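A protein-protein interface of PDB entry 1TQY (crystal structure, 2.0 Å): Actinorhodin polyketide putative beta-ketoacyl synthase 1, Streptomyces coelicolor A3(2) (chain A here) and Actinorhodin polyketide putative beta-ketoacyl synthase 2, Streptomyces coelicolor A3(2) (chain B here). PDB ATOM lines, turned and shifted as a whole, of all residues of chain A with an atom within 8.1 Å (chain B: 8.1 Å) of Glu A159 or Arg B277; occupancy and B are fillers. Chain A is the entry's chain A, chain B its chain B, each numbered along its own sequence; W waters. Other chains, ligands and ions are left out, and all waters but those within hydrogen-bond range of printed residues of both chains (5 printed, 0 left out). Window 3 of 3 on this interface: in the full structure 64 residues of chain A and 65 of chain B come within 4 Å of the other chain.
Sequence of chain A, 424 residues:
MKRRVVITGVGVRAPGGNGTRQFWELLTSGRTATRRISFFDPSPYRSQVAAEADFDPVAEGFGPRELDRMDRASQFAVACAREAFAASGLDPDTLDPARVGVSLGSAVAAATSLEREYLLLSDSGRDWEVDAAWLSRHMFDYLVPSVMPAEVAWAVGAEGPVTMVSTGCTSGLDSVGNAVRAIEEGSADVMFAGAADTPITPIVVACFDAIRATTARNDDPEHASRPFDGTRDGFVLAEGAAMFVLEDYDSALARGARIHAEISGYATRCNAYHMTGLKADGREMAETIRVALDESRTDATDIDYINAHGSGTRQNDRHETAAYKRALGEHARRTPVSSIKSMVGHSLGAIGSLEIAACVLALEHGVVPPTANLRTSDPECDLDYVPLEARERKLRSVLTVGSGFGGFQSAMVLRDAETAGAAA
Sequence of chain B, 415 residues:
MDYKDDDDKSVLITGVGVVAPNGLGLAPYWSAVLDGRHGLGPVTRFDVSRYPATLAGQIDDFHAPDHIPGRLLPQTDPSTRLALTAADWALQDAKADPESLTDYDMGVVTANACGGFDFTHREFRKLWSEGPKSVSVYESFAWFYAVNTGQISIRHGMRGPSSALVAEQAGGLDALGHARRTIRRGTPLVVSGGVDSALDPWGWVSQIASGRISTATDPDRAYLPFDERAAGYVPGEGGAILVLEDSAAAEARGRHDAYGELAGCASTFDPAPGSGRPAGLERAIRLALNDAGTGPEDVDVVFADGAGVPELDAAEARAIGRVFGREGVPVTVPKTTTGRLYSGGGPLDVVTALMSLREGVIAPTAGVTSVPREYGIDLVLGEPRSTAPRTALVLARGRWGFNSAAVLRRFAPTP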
ATOM      1  N   LEU A  95     -14.884 -28.625  21.133  1.00  0.00           N
ATOM      2  CA  LEU A  95     -15.355 -28.420  19.775  1.00  0.00           C
ATOM      3  C   LEU A  95     -15.744 -26.992  19.440  1.00  0.00           C
ATOM      4  O   LEU A  95     -16.340 -26.289  20.254  1.00  0.00           O
ATOM      5  CB  LEU A  95     -16.549 -29.330  19.472  1.00  0.00           C
ATOM      6  CG  LEU A  95     -16.226 -30.735  18.985  1.00  0.00           C
ATOM      7  CD1 LEU A  95     -17.512 -31.475  18.641  1.00  0.00           C
ATOM      8  CD2 LEU A  95     -15.321 -30.637  17.769  1.00  0.00           C
ATOM      9  N   ASP A  96     -15.382 -26.568  18.234  1.00  0.00           N
ATOM     10  CA  ASP A  96     -15.744 -25.250  17.742  1.00  0.00           C
ATOM     11  C   ASP A  96     -16.894 -25.486  16.765  1.00  0.00           C
ATOM     12  O   ASP A  96     -16.676 -25.911  15.627  1.00  0.00           O
ATOM     13  CB  ASP A  96     -14.584 -24.593  17.003  1.00  0.00           C
ATOM     14  CG  ASP A  96     -15.000 -23.301  16.330  1.00  0.00           C
ATOM     15  OD1 ASP A  96     -16.123 -22.833  16.615  1.00  0.00           O
ATOM     16  OD2 ASP A  96     -14.223 -22.742  15.528  1.00  0.00           O
ATOM     17  N   PRO A  97     -18.132 -25.202  17.195  1.00  0.00           N
ATOM     18  CA  PRO A  97     -19.325 -25.389  16.359  1.00  0.00           C
ATOM     19  C   PRO A  97     -19.195 -24.874  14.937  1.00  0.00           C
ATOM     20  O   PRO A  97     -19.778 -25.440  14.026  1.00  0.00           O
ATOM     21  CB  PRO A  97     -20.410 -24.640  17.133  1.00  0.00           C
ATOM     22  CG  PRO A  97     -19.982 -24.800  18.548  1.00  0.00           C
ATOM     23  CD  PRO A  97     -18.489 -24.549  18.469  1.00  0.00           C
ATOM     24  N   ALA A  98     -18.437 -23.800  14.754  1.00  0.00           N
ATOM     25  CA  ALA A  98     -18.280 -23.225  13.433  1.00  0.00           C
ATOM     26  C   ALA A  98     -17.444 -24.119  12.505  1.00  0.00           C
ATOM     27  O   ALA A  98     -17.336 -23.840  11.311  1.00  0.00           O
ATOM     28  CB  ALA A  98     -17.663 -21.831  13.532  1.00  0.00           C
ATOM     29  N   ARG A  99     -16.872 -25.192  13.051  1.00  0.00           N
ATOM     30  CA  ARG A  99     -16.051 -26.107  12.262  1.00  0.00           C
ATOM     31  C   ARG A  99     -16.647 -27.498  12.223  1.00  0.00           C
ATOM     32  O   ARG A  99     -16.003 -28.451  11.784  1.00  0.00           O
ATOM     33  CB  ARG A  99     -14.622 -26.179  12.821  1.00  0.00           C
ATOM     34  CG  ARG A  99     -13.902 -24.841  12.839  1.00  0.00           C
ATOM     35  CD  ARG A  99     -13.767 -24.292  11.426  1.00  0.00           C
ATOM     36  NE  ARG A  99     -12.996 -25.210  10.596  1.00  0.00           N
ATOM     37  CZ  ARG A  99     -12.851 -25.100   9.282  1.00  0.00           C
ATOM     38  NH1 ARG A  99     -13.428 -24.101   8.625  1.00  0.00           N
ATOM     39  NH2 ARG A  99     -12.110 -25.986   8.628  1.00  0.00           N
ATOM     40  N   VAL A 100     -17.883 -27.608  12.687  1.00  0.00           N
ATOM     41  CA  VAL A 100     -18.581 -28.883  12.712  1.00  0.00           C
ATOM     42  C   VAL A 100     -19.749 -28.797  11.749  1.00  0.00           C
ATOM     43  O   VAL A 100     -20.575 -27.893  11.857  1.00  0.00           O
ATOM     44  CB  VAL A 100     -19.103 -29.201  14.124  1.00  0.00           C
ATOM     45  CG1 VAL A 100     -19.904 -30.498  14.104  1.00  0.00           C
ATOM     46  CG2 VAL A 100     -17.929 -29.315  15.073  1.00  0.00           C
ATOM     47  N   GLY A 101     -19.801 -29.724  10.799  1.00  0.00           N
ATOM     48  CA  GLY A 101     -20.874 -29.721   9.826  1.00  0.00           C
ATOM     49  C   GLY A 101     -21.670 -31.008   9.811  1.00  0.00           C
ATOM     50  O   GLY A 101     -21.349 -31.966  10.520  1.00  0.00           O
ATOM     51  N   VAL A 102     -22.710 -31.024   8.988  1.00  0.00           N
ATOM     52  CA  VAL A 102     -23.590 -32.179   8.851  1.00  0.00           C
ATOM     53  C   VAL A 102     -23.904 -32.455   7.375  1.00  0.00           C
ATOM     54  O   VAL A 102     -24.144 -31.531   6.600  1.00  0.00           O
ATOM     55  CB  VAL A 102     -24.932 -31.956   9.591  1.00  0.00           C
ATOM     56  CG1 VAL A 102     -25.892 -33.114   9.285  1.00  0.00           C
ATOM     57  CG2 VAL A 102     -24.690 -31.844  11.090  1.00  0.00           C
ATOM     58  N   ALA A 153     -27.976 -31.501  13.313  1.00  0.00           N
ATOM     59  CA  ALA A 153     -27.066 -30.415  13.641  1.00  0.00           C
ATOM     60  C   ALA A 153     -27.328 -29.855  15.040  1.00  0.00           C
ATOM     61  O   ALA A 153     -26.390 -29.472  15.748  1.00  0.00           O
ATOM     62  CB  ALA A 153     -27.168 -29.294  12.596  1.00  0.00           C
ATOM     63  N   TRP A 154     -28.595 -29.791  15.436  1.00  0.00           N
ATOM     64  CA  TRP A 154     -28.931 -29.287  16.763  1.00  0.00           C
ATOM     65  C   TRP A 154     -28.496 -30.287  17.826  1.00  0.00           C
ATOM     66  O   TRP A 154     -28.096 -29.902  18.922  1.00  0.00           O
ATOM     67  CB  TRP A 154     -30.443 -29.028  16.912  1.00  0.00           C
ATOM     68  CG  TRP A 154     -31.009 -27.983  15.986  1.00  0.00           C
ATOM     69  CD1 TRP A 154     -30.359 -26.895  15.483  1.00  0.00           C
ATOM     70  CD2 TRP A 154     -32.346 -27.920  15.485  1.00  0.00           C
ATOM     71  NE1 TRP A 154     -31.207 -26.156  14.695  1.00  0.00           N
ATOM     72  CE2 TRP A 154     -32.436 -26.764  14.679  1.00  0.00           C
ATOM     73  CE3 TRP A 154     -33.481 -28.730  15.639  1.00  0.00           C
ATOM     74  CZ2 TRP A 154     -33.618 -26.394  14.026  1.00  0.00           C
ATOM     75  CZ3 TRP A 154     -34.652 -28.362  14.991  1.00  0.00           C
ATOM     76  CH2 TRP A 154     -34.707 -27.199  14.192  1.00  0.00           C
ATOM     77  N   VAL A 156     -25.865 -32.370  17.700  1.00  0.00           N
ATOM     78  CA  VAL A 156     -24.408 -32.412  17.808  1.00  0.00           C
ATOM     79  C   VAL A 156     -23.754 -31.050  17.935  1.00  0.00           C
ATOM     80  O   VAL A 156     -22.536 -30.960  18.046  1.00  0.00           O
ATOM     81  CB  VAL A 156     -23.763 -33.112  16.584  1.00  0.00           C
ATOM     82  CG1 VAL A 156     -24.411 -34.445  16.351  1.00  0.00           C
ATOM     83  CG2 VAL A 156     -23.879 -32.220  15.364  1.00  0.00           C
ATOM     84  N   GLY A 157     -24.558 -29.991  17.900  1.00  0.00           N
ATOM     85  CA  GLY A 157     -24.023 -28.645  18.017  1.00  0.00           C
ATOM     86  C   GLY A 157     -23.273 -28.189  16.775  1.00  0.00           C
ATOM     87  O   GLY A 157     -22.263 -27.488  16.866  1.00  0.00           O
ATOM     88  N   ALA A 158     -23.768 -28.575  15.603  1.00  0.00           N
ATOM     89  CA  ALA A 158     -23.117 -28.202  14.348  1.00  0.00           C
ATOM     90  C   ALA A 158     -23.480 -26.801  13.871  1.00  0.00           C
ATOM     91  O   ALA A 158     -24.652 -26.443  13.863  1.00  0.00           O
ATOM     92  CB  ALA A 158     -23.477 -29.215  13.254  1.00  0.00           C
ATOM     93  N   GLU A 159     -22.489 -26.006  13.467  1.00  0.00           N
ATOM     94  CA  GLU A 159     -22.783 -24.671  12.948  1.00  0.00           C
ATOM     95  C   GLU A 159     -22.070 -24.411  11.638  1.00  0.00           C
ATOM     96  O   GLU A 159     -22.148 -23.310  11.088  1.00  0.00           O
ATOM     97  CB  GLU A 159     -22.422 -23.580  13.962  1.00  0.00           C
ATOM     98  CG  GLU A 159     -23.220 -23.692  15.246  1.00  0.00           C
ATOM     99  CD  GLU A 159     -23.156 -22.450  16.117  1.00  0.00           C
ATOM    100  OE1 GLU A 159     -23.365 -22.601  17.330  1.00  0.00           O
ATOM    101  OE2 GLU A 159     -22.918 -21.340  15.592  1.00  0.00           O
ATOM    102  N   GLY A 160     -21.380 -25.433  11.135  1.00  0.00           N
ATOM    103  CA  GLY A 160     -20.679 -25.305   9.868  1.00  0.00           C
ATOM    104  C   GLY A 160     -21.607 -25.672   8.724  1.00  0.00           C
ATOM    105  O   GLY A 160     -22.807 -25.452   8.822  1.00  0.00           O
ATOM    106  N   PRO A 161     -21.080 -26.229   7.622  1.00  0.00           N
ATOM    107  CA  PRO A 161     -21.919 -26.610   6.479  1.00  0.00           C
ATOM    108  C   PRO A 161     -22.874 -27.719   6.880  1.00  0.00           C
ATOM    109  O   PRO A 161     -22.443 -28.790   7.299  1.00  0.00           O
ATOM    110  CB  PRO A 161     -20.900 -27.089   5.443  1.00  0.00           C
ATOM    111  CG  PRO A 161     -19.631 -26.362   5.832  1.00  0.00           C
ATOM    112  CD  PRO A 161     -19.656 -26.469   7.330  1.00  0.00           C
ATOM    113  N   VAL A 162     -24.171 -27.458   6.770  1.00  0.00           N
ATOM    114  CA  VAL A 162     -25.172 -28.459   7.120  1.00  0.00           C
ATOM    115  C   VAL A 162     -26.084 -28.638   5.917  1.00  0.00           C
ATOM    116  O   VAL A 162     -26.651 -27.672   5.413  1.00  0.00           O
ATOM    117  CB  VAL A 162     -26.012 -28.008   8.337  1.00  0.00           C
ATOM    118  CG1 VAL A 162     -27.186 -28.960   8.556  1.00  0.00           C
ATOM    119  CG2 VAL A 162     -25.140 -27.992   9.582  1.00  0.00           C
ATOM    120  N   SER A 187     -13.468 -26.831   4.519  1.00  0.00           N
ATOM    121  CA  SER A 187     -14.727 -26.185   4.889  1.00  0.00           C
ATOM    122  C   SER A 187     -15.221 -26.617   6.263  1.00  0.00           C
ATOM    123  O   SER A 187     -16.158 -26.037   6.807  1.00  0.00           O
ATOM    124  CB  SER A 187     -15.805 -26.494   3.848  1.00  0.00           C
ATOM    125  OG  SER A 187     -15.453 -25.979   2.577  1.00  0.00           O
ATOM    126  N   VAL A 190     -14.724 -31.248  11.477  1.00  0.00           N
ATOM    127  CA  VAL A 190     -15.471 -32.389  11.976  1.00  0.00           C
ATOM    128  C   VAL A 190     -16.799 -32.447  11.219  1.00  0.00           C
ATOM    129  O   VAL A 190     -17.456 -31.423  11.006  1.00  0.00           O
ATOM    130  CB  VAL A 190     -15.724 -32.252  13.493  1.00  0.00           C
ATOM    131  CG1 VAL A 190     -16.398 -33.494  14.036  1.00  0.00           C
ATOM    132  CG2 VAL A 190     -14.398 -32.026  14.207  1.00  0.00           C
ATOM    133  N   SER B 267     -21.290 -21.797   3.258  1.00  0.00           N
ATOM    134  CA  SER B 267     -22.516 -22.235   3.918  1.00  0.00           C
ATOM    135  C   SER B 267     -22.265 -22.377   5.413  1.00  0.00           C
ATOM    136  O   SER B 267     -21.260 -22.959   5.821  1.00  0.00           O
ATOM    137  CB  SER B 267     -22.973 -23.602   3.392  1.00  0.00           C
ATOM    138  OG  SER B 267     -23.289 -23.554   2.015  1.00  0.00           O
ATOM    139  N   THR B 268     -23.163 -21.836   6.230  1.00  0.00           N
ATOM    140  CA  THR B 268     -23.043 -21.966   7.683  1.00  0.00           C
ATOM    141  C   THR B 268     -24.418 -22.375   8.180  1.00  0.00           C
ATOM    142  O   THR B 268     -25.372 -22.413   7.404  1.00  0.00           O
ATOM    143  CB  THR B 268     -22.645 -20.641   8.396  1.00  0.00           C
ATOM    144  OG1 THR B 268     -23.670 -19.661   8.199  1.00  0.00           O
ATOM    145  CG2 THR B 268     -21.309 -20.106   7.874  1.00  0.00           C
ATOM    146  N   PHE B 269     -24.522 -22.710   9.460  1.00  0.00           N
ATOM    147  CA  PHE B 269     -25.801 -23.113  10.029  1.00  0.00           C
ATOM    148  C   PHE B 269     -25.976 -22.433  11.386  1.00  0.00           C
ATOM    149  O   PHE B 269     -25.066 -22.456  12.207  1.00  0.00           O
ATOM    150  CB  PHE B 269     -25.855 -24.636  10.196  1.00  0.00           C
ATOM    151  CG  PHE B 269     -27.229 -25.154  10.515  1.00  0.00           C
ATOM    152  CD1 PHE B 269     -28.259 -25.036   9.586  1.00  0.00           C
ATOM    153  CD2 PHE B 269     -27.508 -25.719  11.750  1.00  0.00           C
ATOM    154  CE1 PHE B 269     -29.557 -25.474   9.883  1.00  0.00           C
ATOM    155  CE2 PHE B 269     -28.805 -26.164  12.066  1.00  0.00           C
ATOM    156  CZ  PHE B 269     -29.829 -26.040  11.129  1.00  0.00           C
ATOM    157  N   ASP B 270     -27.133 -21.824  11.622  1.00  0.00           N
ATOM    158  CA  ASP B 270     -27.365 -21.130  12.892  1.00  0.00           C
ATOM    159  C   ASP B 270     -27.424 -22.076  14.085  1.00  0.00           C
ATOM    160  O   ASP B 270     -27.731 -23.256  13.937  1.00  0.00           O
ATOM    161  CB  ASP B 270     -28.682 -20.343  12.859  1.00  0.00           C
ATOM    162  CG  ASP B 270     -28.682 -19.220  11.838  1.00  0.00           C
ATOM    163  OD1 ASP B 270     -27.601 -18.789  11.392  1.00  0.00           O
ATOM    164  OD2 ASP B 270     -29.781 -18.753  11.493  1.00  0.00           O
ATOM    165  N   PRO B 271     -27.104 -21.571  15.292  1.00  0.00           N
ATOM    166  CA  PRO B 271     -27.159 -22.418  16.484  1.00  0.00           C
ATOM    167  C   PRO B 271     -28.613 -22.769  16.798  1.00  0.00           C
ATOM    168  O   PRO B 271     -29.547 -22.022  16.466  1.00  0.00           O
ATOM    169  CB  PRO B 271     -26.539 -21.539  17.571  1.00  0.00           C
ATOM    170  CG  PRO B 271     -26.851 -20.160  17.103  1.00  0.00           C
ATOM    171  CD  PRO B 271     -26.529 -20.261  15.623  1.00  0.00           C
ATOM    172  N   ALA B 272     -28.787 -23.909  17.449  1.00  0.00           N
ATOM    173  CA  ALA B 272     -30.101 -24.406  17.822  1.00  0.00           C
ATOM    174  C   ALA B 272     -30.985 -23.330  18.448  1.00  0.00           C
ATOM    175  O   ALA B 272     -30.492 -22.387  19.060  1.00  0.00           O
ATOM    176  CB  ALA B 272     -29.947 -25.567  18.785  1.00  0.00           C
ATOM    177  N   PRO B 273     -32.309 -23.454  18.282  1.00  0.00           N
ATOM    178  CA  PRO B 273     -33.243 -22.479  18.852  1.00  0.00           C
ATOM    179  C   PRO B 273     -33.124 -22.449  20.376  1.00  0.00           C
ATOM    180  O   PRO B 273     -33.058 -23.496  21.024  1.00  0.00           O
ATOM    181  CB  PRO B 273     -34.603 -22.992  18.382  1.00  0.00           C
ATOM    182  CG  PRO B 273     -34.279 -23.617  17.049  1.00  0.00           C
ATOM    183  CD  PRO B 273     -33.007 -24.381  17.374  1.00  0.00           C
ATOM    184  N   GLY B 274     -33.089 -21.248  20.942  1.00  0.00           N
ATOM    185  CA  GLY B 274     -32.975 -21.122  22.384  1.00  0.00           C
ATOM    186  C   GLY B 274     -31.562 -20.864  22.878  1.00  0.00           C
ATOM    187  O   GLY B 274     -31.362 -20.404  24.004  1.00  0.00           O
ATOM    188  N   SER B 275     -30.575 -21.161  22.040  1.00  0.00           N
ATOM    189  CA  SER B 275     -29.184 -20.951  22.418  1.00  0.00           C
ATOM    190  C   SER B 275     -28.878 -19.465  22.588  1.00  0.00           C
ATOM    191  O   SER B 275     -27.911 -19.094  23.258  1.00  0.00           O
ATOM    192  CB  SER B 275     -28.250 -21.522  21.354  1.00  0.00           C
ATOM    193  OG  SER B 275     -28.395 -20.805  20.141  1.00  0.00           O
ATOM    194  N   GLY B 276     -29.698 -18.619  21.973  1.00  0.00           N
ATOM    195  CA  GLY B 276     -29.481 -17.188  22.070  1.00  0.00           C
ATOM    196  C   GLY B 276     -28.259 -16.727  21.293  1.00  0.00           C
ATOM    197  O   GLY B 276     -28.138 -15.547  20.966  1.00  0.00           O
ATOM    198  N   ARG B 277     -27.348 -17.654  20.999  1.00  0.00           N
ATOM    199  CA  ARG B 277     -26.139 -17.325  20.249  1.00  0.00           C
ATOM    200  C   ARG B 277     -26.541 -16.657  18.937  1.00  0.00           C
ATOM    201  O   ARG B 277     -27.640 -16.878  18.421  1.00  0.00           O
ATOM    202  CB  ARG B 277     -25.321 -18.584  19.969  1.00  0.00           C
ATOM    203  CG  ARG B 277     -25.067 -19.423  21.201  1.00  0.00           C
ATOM    204  CD  ARG B 277     -24.733 -20.876  20.852  1.00  0.00           C
ATOM    205  NE  ARG B 277     -23.310 -21.112  20.621  1.00  0.00           N
ATOM    206  CZ  ARG B 277     -22.618 -20.672  19.573  1.00  0.00           C
ATOM    207  NH1 ARG B 277     -23.213 -19.958  18.626  1.00  0.00           N
ATOM    208  NH2 ARG B 277     -21.323 -20.955  19.472  1.00  0.00           N
ATOM    209  N   PRO B 278     -25.650 -15.835  18.374  1.00  0.00           N
ATOM    210  CA  PRO B 278     -25.931 -15.134  17.119  1.00  0.00           C
ATOM    211  C   PRO B 278     -26.065 -16.044  15.894  1.00  0.00           C
ATOM    212  O   PRO B 278     -25.523 -17.151  15.864  1.00  0.00           O
ATOM    213  CB  PRO B 278     -24.752 -14.179  17.000  1.00  0.00           C
ATOM    214  CG  PRO B 278     -23.629 -14.998  17.564  1.00  0.00           C
ATOM    215  CD  PRO B 278     -24.256 -15.611  18.801  1.00  0.00           C
ATOM    216  N   ALA B 279     -26.801 -15.559  14.895  1.00  0.00           N
ATOM    217  CA  ALA B 279     -27.012 -16.286  13.650  1.00  0.00           C
ATOM    218  C   ALA B 279     -25.680 -16.402  12.937  1.00  0.00           C
ATOM    219  O   ALA B 279     -24.736 -15.682  13.261  1.00  0.00           O
ATOM    220  CB  ALA B 279     -28.005 -15.549  12.766  1.00  0.00           C
ATOM    221  N   GLY B 280     -25.605 -17.307  11.964  1.00  0.00           N
ATOM    222  CA  GLY B 280     -24.365 -17.500  11.228  1.00  0.00           C
ATOM    223  C   GLY B 280     -24.312 -16.844   9.856  1.00  0.00           C
ATOM    224  O   GLY B 280     -23.432 -17.169   9.062  1.00  0.00           O
ATOM    225  N   ARG B 283     -21.089 -14.743   9.445  1.00  0.00           N
ATOM    226  CA  ARG B 283     -19.970 -15.647   9.210  1.00  0.00           C
ATOM    227  C   ARG B 283     -19.934 -16.163   7.762  1.00  0.00           C
ATOM    228  O   ARG B 283     -18.872 -16.174   7.136  1.00  0.00           O
ATOM    229  CB  ARG B 283     -19.998 -16.831  10.189  1.00  0.00           C
ATOM    230  CG  ARG B 283     -18.841 -17.823   9.985  1.00  0.00           C
ATOM    231  CD  ARG B 283     -18.636 -18.780  11.167  1.00  0.00           C
ATOM    232  NE  ARG B 283     -19.675 -19.806  11.282  1.00  0.00           N
ATOM    233  CZ  ARG B 283     -20.833 -19.635  11.909  1.00  0.00           C
ATOM    234  NH1 ARG B 283     -21.106 -18.471  12.488  1.00  0.00           N
ATOM    235  NH2 ARG B 283     -21.717 -20.624  11.948  1.00  0.00           N
ATOM    236  N   ALA B 284     -21.083 -16.582   7.232  1.00  0.00           N
ATOM    237  CA  ALA B 284     -21.137 -17.080   5.859  1.00  0.00           C
ATOM    238  C   ALA B 284     -20.617 -16.021   4.891  1.00  0.00           C
ATOM    239  O   ALA B 284     -19.814 -16.310   4.001  1.00  0.00           O
ATOM    240  CB  ALA B 284     -22.583 -17.470   5.483  1.00  0.00           C
ATOM    241  N   LEU B 287     -16.935 -15.648   5.113  1.00  0.00           N
ATOM    242  CA  LEU B 287     -16.296 -16.863   4.622  1.00  0.00           C
ATOM    243  C   LEU B 287     -16.276 -16.798   3.098  1.00  0.00           C
ATOM    244  O   LEU B 287     -15.258 -17.066   2.465  1.00  0.00           O
ATOM    245  CB  LEU B 287     -17.065 -18.101   5.089  1.00  0.00           C
ATOM    246  CG  LEU B 287     -16.405 -19.011   6.128  1.00  0.00           C
ATOM    247  CD1 LEU B 287     -15.486 -18.227   7.038  1.00  0.00           C
ATOM    248  CD2 LEU B 287     -17.486 -19.746   6.912  1.00  0.00           C
ATOM    249  N   GLY B 401     -32.393 -22.271   9.884  1.00  0.00           N
ATOM    250  CA  GLY B 401     -31.039 -21.778  10.074  1.00  0.00           C
ATOM    251  C   GLY B 401     -29.986 -21.881   8.991  1.00  0.00           C
ATOM    252  O   GLY B 401     -28.837 -21.511   9.234  1.00  0.00           O
ATOM    253  N   ASN B 403     -27.666 -20.926   6.037  1.00  0.00           N
ATOM    254  CA  ASN B 403     -27.112 -19.697   5.484  1.00  0.00           C
ATOM    255  C   ASN B 403     -26.248 -19.999   4.284  1.00  0.00           C
ATOM    256  O   ASN B 403     -25.505 -20.977   4.280  1.00  0.00           O
ATOM    257  CB  ASN B 403     -26.249 -18.979   6.517  1.00  0.00           C
ATOM    258  CG  ASN B 403     -27.031 -18.556   7.715  1.00  0.00           C
ATOM    259  OD1 ASN B 403     -27.988 -17.806   7.601  1.00  0.00           O
ATOM    260  ND2 ASN B 403     -26.640 -19.049   8.877  1.00  0.00           N
HETATM  261  O   HOH W   1     -30.587 -23.756  13.582  1.00  0.00           O
HETATM  262  O   HOH W   2     -23.857 -20.011  13.209  1.00  0.00           O
HETATM  263  O   HOH W   3     -27.010 -25.551  15.289  1.00  0.00           O
HETATM  264  O   HOH W   4     -18.768 -22.017   9.976  1.00  0.00           O
HETATM  265  O   HOH W   5     -25.256 -24.890   5.732  1.00  0.00           O
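CB of Ala A98 touches NE of Arg B283 (3.6 Å).
CB of Ala A153 touches CE2 of Phe B269, at 3.6 Å.
CE2 of Phe B269 touches NE1 of Trp A154, at 3.6 Å.
CA of Ala B272 touches CD1 of Trp A154 (3.4 Å).
Trp A154 touches Pro B273 (CE2 to CD, 3.6 Å).
Ala A158 touches Phe B269 (O to CD2, 3.6 Å).
Gly A160 touches Ser B267.
Thr B268 touches Gly A160 (C to O, 3.5 Å).
Pro A161 touches Ser B267.
CG2 of Val A162 touches CB of Phe B269, 3.5 Å away.
The backbone carbonyl oxygen (O) of Pro A97 sits at hydrogen-bond distance from the backbone NH (N) of Glu A159 (2.8 Å).
O of Pro A97 sits at hydrogen-bond distance from N of Gly A160 (3.3 Å).
The backbone carbonyl oxygen (O) of Val A100 lies within hydrogen-bond range of the backbone NH (N) of Gly A160 (2.7 Å).
The backbone carbonyl oxygen of Ala A153 lies within hydrogen-bond range of the backbone NH of Ala A158 (2.8 Å).
The side-chain hydroxyl (OG1) of Thr B268 sits at hydrogen-bond distance from the backbone carbonyl oxygen (O) of Gly B280 (2.6 Å).
The backbone carbonyl oxygen (O) of Ala B272 lies within hydrogen-bond range of the side-chain hydroxyl (OG) of Ser B275 (2.8 Å).
Among the printed residues, Asp or Glu carboxylates within 4 Å of a Lys or Arg side-chain nitrogen of the other chain: Glu A159 with Arg B277 (2.9 Å) and Glu A159 with Arg B283 (3.9 Å).
Glu A159 touches just these residues of chain B: Thr B268, Phe B269, Pro B271, Arg B277 and Arg B283.
Of chain A, only Glu A159 comes within 4 Å of Arg B277.
Of chain B, only Phe B269 (3.6 Å) comes within 4 Å of Ala A158.
No residue of chain A comes within 4 Å of Gly B276.
No residue of chain A comes within 4 Å of Pro B278.
Printed residues of chain A within 4 Å of Thr B268: Glu A159 (3.8 Å) and Gly A160 (3.5 Å).
Of the printed residues of chain B, Ala A153 touches Phe B269.
Of the printed residues of chain A, Phe B269 touches Ala A153, Trp A154, Ala A158, Glu A159, Gly A160 and Val A162.
Of the printed residues of chain A, Ala B272 touches Trp A154 (3.4 Å).
Leu B287 touches none of the printed residues of chain A.
The nearest residue of chain B that does not touch Glu A159 is Asp B270 (4.7 Å).
The nearest printed residue of chain A that does not touch Arg B283 is Gly A160 (4.9 Å).
Water W2 lies within hydrogen-bond range of the guanidinium group of Arg B283, the side-chain carboxylate of Glu A159, the backbone carbonyl oxygen of Phe B269 and the backbone NH of Gly B280.
Water W4 bridges O of Ala A98 (2.7 Å) and NE of Arg B283 (2.7 Å).
Water W1 lies within hydrogen-bond range of the indole nitrogen (NE1) of Trp A154 (2.7 Å) and the backbone carbonyl oxygen (O) of Asp B270 (2.9 Å).
Water W3 lies within hydrogen-bond range of the backbone carbonyl oxygen (O) of Asp B270 (2.8 Å), the backbone carbonyl oxygen (O) of Ala A158 (2.9 Å) and the backbone NH (N) of Ala B272 (3.2 Å).
Water W5 bridges the backbone NH (N) of Val A162 (3.0 Å) and the backbone carbonyl oxygen (O) of Thr B268 (3.0 Å).
O of Glu A159 sits at hydrogen-bond distance from N of Phe B269 (2.9 Å).
The side-chain carboxylate (OE1) of Glu A159 lies within salt-bridge range of the guanidinium group (NH1) of Arg B277 (2.9 Å).
OE2 of Glu A159 lies within salt-bridge range of NH2 of Arg B283.
The backbone carbonyl oxygen (O) of Gly A160 sits at hydrogen-bond distance from the backbone NH (N) of Phe B269 (3.3 Å).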
